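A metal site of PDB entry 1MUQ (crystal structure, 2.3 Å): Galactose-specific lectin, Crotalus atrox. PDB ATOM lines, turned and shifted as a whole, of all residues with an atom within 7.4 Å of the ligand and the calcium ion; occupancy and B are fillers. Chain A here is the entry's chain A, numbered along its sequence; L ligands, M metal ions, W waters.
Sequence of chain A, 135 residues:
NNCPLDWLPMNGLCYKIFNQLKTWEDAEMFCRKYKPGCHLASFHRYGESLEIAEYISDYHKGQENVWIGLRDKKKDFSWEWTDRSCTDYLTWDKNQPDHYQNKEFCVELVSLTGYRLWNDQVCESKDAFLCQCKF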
ATOM      1  N   ASN A  65     -18.219   2.671 -25.736  1.00  0.00           N
ATOM      2  CA  ASN A  65     -17.607   3.403 -26.817  1.00  0.00           C
ATOM      3  C   ASN A  65     -17.865   2.609 -28.105  1.00  0.00           C
ATOM      4  O   ASN A  65     -18.246   1.427 -28.048  1.00  0.00           O
ATOM      5  CB  ASN A  65     -16.108   3.573 -26.595  1.00  0.00           C
ATOM      6  CG  ASN A  65     -15.808   4.364 -25.338  1.00  0.00           C
ATOM      7  OD1 ASN A  65     -16.517   5.312 -24.990  1.00  0.00           O
ATOM      8  ND2 ASN A  65     -14.738   3.984 -24.651  1.00  0.00           N
ATOM      9  N   TRP A  92      -9.491  13.646 -32.842  1.00  0.00           N
ATOM     10  CA  TRP A  92      -9.067  12.991 -31.627  1.00  0.00           C
ATOM     11  C   TRP A  92      -9.577  13.683 -30.381  1.00  0.00           C
ATOM     12  O   TRP A  92      -9.788  14.891 -30.376  1.00  0.00           O
ATOM     13  CB  TRP A  92      -7.538  12.944 -31.548  1.00  0.00           C
ATOM     14  CG  TRP A  92      -6.921  12.124 -32.628  1.00  0.00           C
ATOM     15  CD1 TRP A  92      -6.261  12.584 -33.726  1.00  0.00           C
ATOM     16  CD2 TRP A  92      -6.924  10.695 -32.716  1.00  0.00           C
ATOM     17  NE1 TRP A  92      -5.854  11.526 -34.505  1.00  0.00           N
ATOM     18  CE2 TRP A  92      -6.246  10.349 -33.904  1.00  0.00           C
ATOM     19  CE3 TRP A  92      -7.435   9.672 -31.908  1.00  0.00           C
ATOM     20  CZ2 TRP A  92      -6.064   9.034 -34.303  1.00  0.00           C
ATOM     21  CZ3 TRP A  92      -7.251   8.366 -32.309  1.00  0.00           C
ATOM     22  CH2 TRP A  92      -6.566   8.050 -33.496  1.00  0.00           C
ATOM     23  N   ASP A  93      -9.793  12.898 -29.333  1.00  0.00           N
ATOM     24  CA  ASP A  93     -10.256  13.433 -28.068  1.00  0.00           C
ATOM     25  C   ASP A  93      -9.058  14.075 -27.389  1.00  0.00           C
ATOM     26  O   ASP A  93      -7.920  13.915 -27.843  1.00  0.00           O
ATOM     27  CB  ASP A  93     -10.810  12.315 -27.200  1.00  0.00           C
ATOM     28  CG  ASP A  93     -11.543  12.843 -25.985  1.00  0.00           C
ATOM     29  OD1 ASP A  93     -11.705  14.079 -25.884  1.00  0.00           O
ATOM     30  OD2 ASP A  93     -11.946  12.011 -25.141  1.00  0.00           O
ATOM     31  N   LYS A  94      -9.308  14.793 -26.305  1.00  0.00           N
ATOM     32  CA  LYS A  94      -8.232  15.453 -25.583  1.00  0.00           C
ATOM     33  C   LYS A  94      -7.177  14.451 -25.141  1.00  0.00           C
ATOM     34  O   LYS A  94      -7.507  13.423 -24.531  1.00  0.00           O
ATOM     35  CB  LYS A  94      -8.810  16.181 -24.357  1.00  0.00           C
ATOM     36  CG  LYS A  94      -7.809  17.071 -23.631  1.00  0.00           C
ATOM     37  CD  LYS A  94      -8.466  17.759 -22.438  1.00  0.00           C
ATOM     38  CE  LYS A  94      -7.494  18.646 -21.698  1.00  0.00           C
ATOM     39  NZ  LYS A  94      -8.120  19.261 -20.495  1.00  0.00           N
ATOM     40  N   ASN A  95      -5.918  14.733 -25.467  1.00  0.00           N
ATOM     41  CA  ASN A  95      -4.790  13.888 -25.102  1.00  0.00           C
ATOM     42  C   ASN A  95      -4.702  12.582 -25.884  1.00  0.00           C
ATOM     43  O   ASN A  95      -4.095  11.617 -25.417  1.00  0.00           O
ATOM     44  CB  ASN A  95      -4.859  13.560 -23.614  1.00  0.00           C
ATOM     45  CG  ASN A  95      -4.742  14.777 -22.743  1.00  0.00           C
ATOM     46  OD1 ASN A  95      -5.126  14.756 -21.569  1.00  0.00           O
ATOM     47  ND2 ASN A  95      -4.218  15.864 -23.299  1.00  0.00           N
ATOM     48  N   GLN A  96      -5.295  12.549 -27.068  1.00  0.00           N
ATOM     49  CA  GLN A  96      -5.260  11.348 -27.879  1.00  0.00           C
ATOM     50  C   GLN A  96      -4.783  11.725 -29.278  1.00  0.00           C
ATOM     51  O   GLN A  96      -4.856  12.889 -29.655  1.00  0.00           O
ATOM     52  CB  GLN A  96      -6.653  10.721 -27.952  1.00  0.00           C
ATOM     53  CG  GLN A  96      -7.330  10.482 -26.607  1.00  0.00           C
ATOM     54  CD  GLN A  96      -6.622   9.460 -25.739  1.00  0.00           C
ATOM     55  OE1 GLN A  96      -5.809   8.671 -26.223  1.00  0.00           O
ATOM     56  NE2 GLN A  96      -6.937   9.461 -24.443  1.00  0.00           N
ATOM     57  N   PRO A  97      -4.273  10.767 -30.057  1.00  0.00           N
ATOM     58  CA  PRO A  97      -4.086   9.351 -29.709  1.00  0.00           C
ATOM     59  C   PRO A  97      -2.808   9.249 -28.882  1.00  0.00           C
ATOM     60  O   PRO A  97      -1.850   9.980 -29.127  1.00  0.00           O
ATOM     61  CB  PRO A  97      -3.961   8.694 -31.070  1.00  0.00           C
ATOM     62  CG  PRO A  97      -3.182   9.709 -31.847  1.00  0.00           C
ATOM     63  CD  PRO A  97      -3.838  11.030 -31.437  1.00  0.00           C
ATOM     64  N   ASP A  98      -2.794   8.351 -27.909  1.00  0.00           N
ATOM     65  CA  ASP A  98      -1.614   8.235 -27.066  1.00  0.00           C
ATOM     66  C   ASP A  98      -0.924   6.882 -27.014  1.00  0.00           C
ATOM     67  O   ASP A  98       0.040   6.731 -26.264  1.00  0.00           O
ATOM     68  CB  ASP A  98      -1.949   8.648 -25.637  1.00  0.00           C
ATOM     69  CG  ASP A  98      -3.037   7.799 -25.027  1.00  0.00           C
ATOM     70  OD1 ASP A  98      -3.419   6.779 -25.640  1.00  0.00           O
ATOM     71  OD2 ASP A  98      -3.510   8.145 -23.935  1.00  0.00           O
ATOM     72  N   HIS A  99      -1.390   5.912 -27.799  1.00  0.00           N
ATOM     73  CA  HIS A  99      -0.786   4.584 -27.778  1.00  0.00           C
ATOM     74  C   HIS A  99      -0.498   4.210 -26.316  1.00  0.00           C
ATOM     75  O   HIS A  99       0.606   3.766 -25.981  1.00  0.00           O
ATOM     76  CB  HIS A  99       0.527   4.583 -28.570  1.00  0.00           C
ATOM     77  CG  HIS A  99       0.348   4.480 -30.049  1.00  0.00           C
ATOM     78  ND1 HIS A  99       1.404   4.349 -30.920  1.00  0.00           N
ATOM     79  CD2 HIS A  99      -0.777   4.461 -30.815  1.00  0.00           C
ATOM     80  CE1 HIS A  99       0.942   4.254 -32.154  1.00  0.00           C
ATOM     81  NE2 HIS A  99      -0.378   4.321 -32.123  1.00  0.00           N
ATOM     82  N   TYR A 100      -1.491   4.409 -25.466  1.00  0.00           N
ATOM     83  CA  TYR A 100      -1.349   4.116 -24.052  1.00  0.00           C
ATOM     84  C   TYR A 100      -0.664   2.771 -23.807  1.00  0.00           C
ATOM     85  O   TYR A 100      -1.162   1.713 -24.224  1.00  0.00           O
ATOM     86  CB  TYR A 100      -2.724   4.133 -23.390  1.00  0.00           C
ATOM     87  CG  TYR A 100      -2.684   4.044 -21.887  1.00  0.00           C
ATOM     88  CD1 TYR A 100      -3.428   3.080 -21.216  1.00  0.00           C
ATOM     89  CD2 TYR A 100      -1.918   4.940 -21.141  1.00  0.00           C
ATOM     90  CE1 TYR A 100      -3.411   3.005 -19.828  1.00  0.00           C
ATOM     91  CE2 TYR A 100      -1.899   4.876 -19.756  1.00  0.00           C
ATOM     92  CZ  TYR A 100      -2.652   3.908 -19.102  1.00  0.00           C
ATOM     93  OH  TYR A 100      -2.665   3.833 -17.733  1.00  0.00           O
ATOM     94  N   GLN A 101       0.485   2.833 -23.141  1.00  0.00           N
ATOM     95  CA  GLN A 101       1.270   1.638 -22.827  1.00  0.00           C
ATOM     96  C   GLN A 101       1.647   0.823 -24.053  1.00  0.00           C
ATOM     97  O   GLN A 101       1.916  -0.376 -23.953  1.00  0.00           O
ATOM     98  CB  GLN A 101       0.514   0.772 -21.820  1.00  0.00           C
ATOM     99  CG  GLN A 101       0.402   1.392 -20.435  1.00  0.00           C
ATOM    100  CD  GLN A 101      -0.383   0.519 -19.470  1.00  0.00           C
ATOM    101  OE1 GLN A 101      -0.141  -0.679 -19.380  1.00  0.00           O
ATOM    102  NE2 GLN A 101      -1.314   1.128 -18.738  1.00  0.00           N
ATOM    103  N   GLU A 104      -2.521   0.393 -27.596  1.00  0.00           N
ATOM    104  CA  GLU A 104      -3.729   0.922 -28.223  1.00  0.00           C
ATOM    105  C   GLU A 104      -3.444   1.366 -29.667  1.00  0.00           C
ATOM    106  O   GLU A 104      -2.664   2.302 -29.901  1.00  0.00           O
ATOM    107  CB  GLU A 104      -4.266   2.084 -27.391  1.00  0.00           C
ATOM    108  CG  GLU A 104      -4.735   1.662 -25.999  1.00  0.00           C
ATOM    109  CD  GLU A 104      -5.301   2.807 -25.172  1.00  0.00           C
ATOM    110  OE1 GLU A 104      -6.042   2.545 -24.197  1.00  0.00           O
ATOM    111  OE2 GLU A 104      -4.979   3.973 -25.489  1.00  0.00           O
ATOM    112  N   CYS A 106      -6.311   0.851 -32.105  1.00  0.00           N
ATOM    113  CA  CYS A 106      -7.634   0.823 -32.729  1.00  0.00           C
ATOM    114  C   CYS A 106      -8.459   1.970 -32.195  1.00  0.00           C
ATOM    115  O   CYS A 106      -8.479   2.240 -30.990  1.00  0.00           O
ATOM    116  CB  CYS A 106      -8.310  -0.523 -32.456  1.00  0.00           C
ATOM    117  SG  CYS A 106      -7.533  -1.895 -33.362  1.00  0.00           S
ATOM    118  N   GLU A 108     -11.858   4.264 -31.431  1.00  0.00           N
ATOM    119  CA  GLU A 108     -13.242   4.168 -31.013  1.00  0.00           C
ATOM    120  C   GLU A 108     -13.814   5.575 -30.795  1.00  0.00           C
ATOM    121  O   GLU A 108     -13.077   6.527 -30.539  1.00  0.00           O
ATOM    122  CB  GLU A 108     -13.331   3.392 -29.700  1.00  0.00           C
ATOM    123  CG  GLU A 108     -12.742   4.157 -28.508  1.00  0.00           C
ATOM    124  CD  GLU A 108     -12.662   3.334 -27.244  1.00  0.00           C
ATOM    125  OE1 GLU A 108     -12.294   3.896 -26.189  1.00  0.00           O
ATOM    126  OE2 GLU A 108     -12.951   2.122 -27.292  1.00  0.00           O
ATOM    127  N   VAL A 110     -15.580   8.011 -28.463  1.00  0.00           N
ATOM    128  CA  VAL A 110     -15.714   8.086 -27.021  1.00  0.00           C
ATOM    129  C   VAL A 110     -17.102   8.518 -26.578  1.00  0.00           C
ATOM    130  O   VAL A 110     -17.593   9.603 -26.921  1.00  0.00           O
ATOM    131  CB  VAL A 110     -14.648   9.035 -26.438  1.00  0.00           C
ATOM    132  CG1 VAL A 110     -14.751   9.062 -24.923  1.00  0.00           C
ATOM    133  CG2 VAL A 110     -13.266   8.570 -26.850  1.00  0.00           C
ATOM    134  N   LEU A 112     -18.167   9.453 -23.666  1.00  0.00           N
ATOM    135  CA  LEU A 112     -18.211  10.636 -22.814  1.00  0.00           C
ATOM    136  C   LEU A 112     -18.234  11.938 -23.600  1.00  0.00           C
ATOM    137  O   LEU A 112     -18.668  12.967 -23.072  1.00  0.00           O
ATOM    138  CB  LEU A 112     -17.012  10.654 -21.848  1.00  0.00           C
ATOM    139  CG  LEU A 112     -17.038   9.664 -20.682  1.00  0.00           C
ATOM    140  CD1 LEU A 112     -15.785   9.841 -19.839  1.00  0.00           C
ATOM    141  CD2 LEU A 112     -18.291   9.908 -19.840  1.00  0.00           C
ATOM    142  N   TRP A 118     -12.516  10.935 -30.957  1.00  0.00           N
ATOM    143  CA  TRP A 118     -11.872   9.627 -31.038  1.00  0.00           C
ATOM    144  C   TRP A 118     -10.783   9.373 -30.013  1.00  0.00           C
ATOM    145  O   TRP A 118     -10.120  10.301 -29.527  1.00  0.00           O
ATOM    146  CB  TRP A 118     -11.220   9.437 -32.401  1.00  0.00           C
ATOM    147  CG  TRP A 118     -12.061   9.808 -33.566  1.00  0.00           C
ATOM    148  CD1 TRP A 118     -13.423   9.948 -33.597  1.00  0.00           C
ATOM    149  CD2 TRP A 118     -11.594  10.028 -34.896  1.00  0.00           C
ATOM    150  NE1 TRP A 118     -13.830  10.241 -34.874  1.00  0.00           N
ATOM    151  CE2 TRP A 118     -12.739  10.295 -35.695  1.00  0.00           C
ATOM    152  CE3 TRP A 118     -10.339  10.011 -35.501  1.00  0.00           C
ATOM    153  CZ2 TRP A 118     -12.644  10.558 -37.059  1.00  0.00           C
ATOM    154  CZ3 TRP A 118     -10.240  10.275 -36.856  1.00  0.00           C
ATOM    155  CH2 TRP A 118     -11.392  10.542 -37.618  1.00  0.00           C
ATOM    156  N   ASN A 119     -10.579   8.094 -29.732  1.00  0.00           N
ATOM    157  CA  ASN A 119      -9.551   7.667 -28.803  1.00  0.00           C
ATOM    158  C   ASN A 119      -8.943   6.351 -29.303  1.00  0.00           C
ATOM    159  O   ASN A 119      -9.680   5.448 -29.691  1.00  0.00           O
ATOM    160  CB  ASN A 119     -10.125   7.448 -27.410  1.00  0.00           C
ATOM    161  CG  ASN A 119      -9.178   6.693 -26.504  1.00  0.00           C
ATOM    162  OD1 ASN A 119      -8.029   7.076 -26.337  1.00  0.00           O
ATOM    163  ND2 ASN A 119      -9.650   5.595 -25.925  1.00  0.00           N
ATOM    164  N   ASP A 120      -7.620   6.249 -29.306  1.00  0.00           N
ATOM    165  CA  ASP A 120      -7.003   5.004 -29.722  1.00  0.00           C
ATOM    166  C   ASP A 120      -7.214   4.102 -28.518  1.00  0.00           C
ATOM    167  O   ASP A 120      -7.025   4.505 -27.371  1.00  0.00           O
ATOM    168  CB  ASP A 120      -5.526   5.192 -30.056  1.00  0.00           C
ATOM    169  CG  ASP A 120      -4.762   5.923 -28.984  1.00  0.00           C
ATOM    170  OD1 ASP A 120      -5.407   6.565 -28.126  1.00  0.00           O
ATOM    171  OD2 ASP A 120      -3.519   5.857 -29.012  1.00  0.00           O
ATOM    172  N   GLN A 121      -7.642   2.877 -28.779  1.00  0.00           N
ATOM    173  CA  GLN A 121      -7.975   1.940 -27.735  1.00  0.00           C
ATOM    174  C   GLN A 121      -7.327   0.587 -27.989  1.00  0.00           C
ATOM    175  O   GLN A 121      -6.920   0.272 -29.122  1.00  0.00           O
ATOM    176  CB  GLN A 121      -9.510   1.803 -27.721  1.00  0.00           C
ATOM    177  CG  GLN A 121     -10.097   0.944 -26.639  1.00  0.00           C
ATOM    178  CD  GLN A 121      -9.579   1.323 -25.283  1.00  0.00           C
ATOM    179  OE1 GLN A 121      -8.555   0.797 -24.828  1.00  0.00           O
ATOM    180  NE2 GLN A 121     -10.259   2.271 -24.634  1.00  0.00           N
ATOM    181  N   VAL A 122      -7.222  -0.196 -26.924  1.00  0.00           N
ATOM    182  CA  VAL A 122      -6.667  -1.536 -27.012  1.00  0.00           C
ATOM    183  C   VAL A 122      -7.597  -2.259 -27.983  1.00  0.00           C
ATOM    184  O   VAL A 122      -8.810  -2.323 -27.754  1.00  0.00           O
ATOM    185  CB  VAL A 122      -6.685  -2.223 -25.638  1.00  0.00           C
ATOM    186  CG1 VAL A 122      -6.408  -3.690 -25.805  1.00  0.00           C
ATOM    187  CG2 VAL A 122      -5.674  -1.553 -24.706  1.00  0.00           C
HETATM  188  C1  LIG L   1      -8.481   7.206 -21.395  1.00  0.00           C
HETATM  189  C2  LIG L   1      -8.485   6.384 -22.697  1.00  0.00           C
HETATM  190  C3  LIG L   1      -7.361   5.332 -22.694  1.00  0.00           C
HETATM  191  C4  LIG L   1      -6.025   5.923 -22.262  1.00  0.00           C
HETATM  192  C5  LIG L   1      -6.178   6.750 -20.987  1.00  0.00           C
HETATM  193  C6  LIG L   1      -4.915   7.436 -20.549  1.00  0.00           C
HETATM  194  O1  LIG L   1      -9.398   8.249 -21.483  1.00  0.00           O
HETATM  195  O2  LIG L   1      -9.732   5.731 -22.834  1.00  0.00           O
HETATM  196  O3  LIG L   1      -7.222   4.822 -24.001  1.00  0.00           O
HETATM  197  O4  LIG L   1      -5.513   6.739 -23.312  1.00  0.00           O
HETATM  198  O5  LIG L   1      -7.177   7.768 -21.177  1.00  0.00           O
HETATM  199  O6  LIG L   1      -4.741   7.325 -19.139  1.00  0.00           O
HETATM  200 CA    CA M   1      -5.869   6.272 -25.986  1.00  0.00          CA
HETATM  201  O   HOH W   1     -11.296   7.852 -23.864  1.00  0.00           O
HETATM  202  O   HOH W   2      -6.098   9.800 -19.526  1.00  0.00           O
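The side-chain carboxylate (OD1) of Asp 120 is bound to the calcium ion. OD1 of Asn 119 binds the calcium ion (2.3 Å). OE1 of Gln 96 binds the calcium ion (2.4 Å). The calcium ion is bound by the side-chain carboxylate (OE2) of Glu 104 (2.5 Å). The calcium ion is bound by the backbone carbonyl oxygen (O) of Asp 120, at 2.5 Å. The calcium ion is bound by the side-chain carboxylate (OD1) of Asp 98. O4 of the ligand binds the calcium ion, at 2.7 Å. The calcium ion is bound by O3 of the ligand (2.8 Å).
The side-chain carboxylate (OD2) of Asp 120 lies within hydrogen-bond range of the backbone NH (N) of His 99, 2.5 Å away. O of Asn 119 is in hydrogen-bond range of N of Glu 108. OE1 of Glu 104 sits close to OE1 of Gln 121, 3.1 Å away. The backbone NH (N) of Tyr 100 lies close to the side-chain carboxylate (OD1) of Asp 98 (3.1 Å). The side-chain amide nitrogen (NE2) of Gln 101 sits close to the side-chain hydroxyl (OH) of Tyr 100 (3.2 Å). The side-chain carboxylate (OE1) of Glu 108 sits at hydrogen-bond distance from the side-chain amide nitrogen (NE2) of Gln 121, 3.0 Å away. The backbone NH (N) of Gln 121 lies within hydrogen-bond range of the backbone carbonyl oxygen (O) of Cys 106, at 2.4 Å.
Of the 21 residues printed, 5 come within 4 Å of the calcium ion.
Water W1 bridges an oxygen (O2) of the ligand and the side-chain amide nitrogen of Asn 119.
Residues that only touch the ligand: Tyr 100 and Gln 121. Hydrophobic or aromatic side chains within 4 Å of the ligand: Tyr 100. Of the 21 residues printed, 7 come within 4 Å of the ligand. Along chain A the residues within 4 Å of the ligand span positions 96 to 121.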
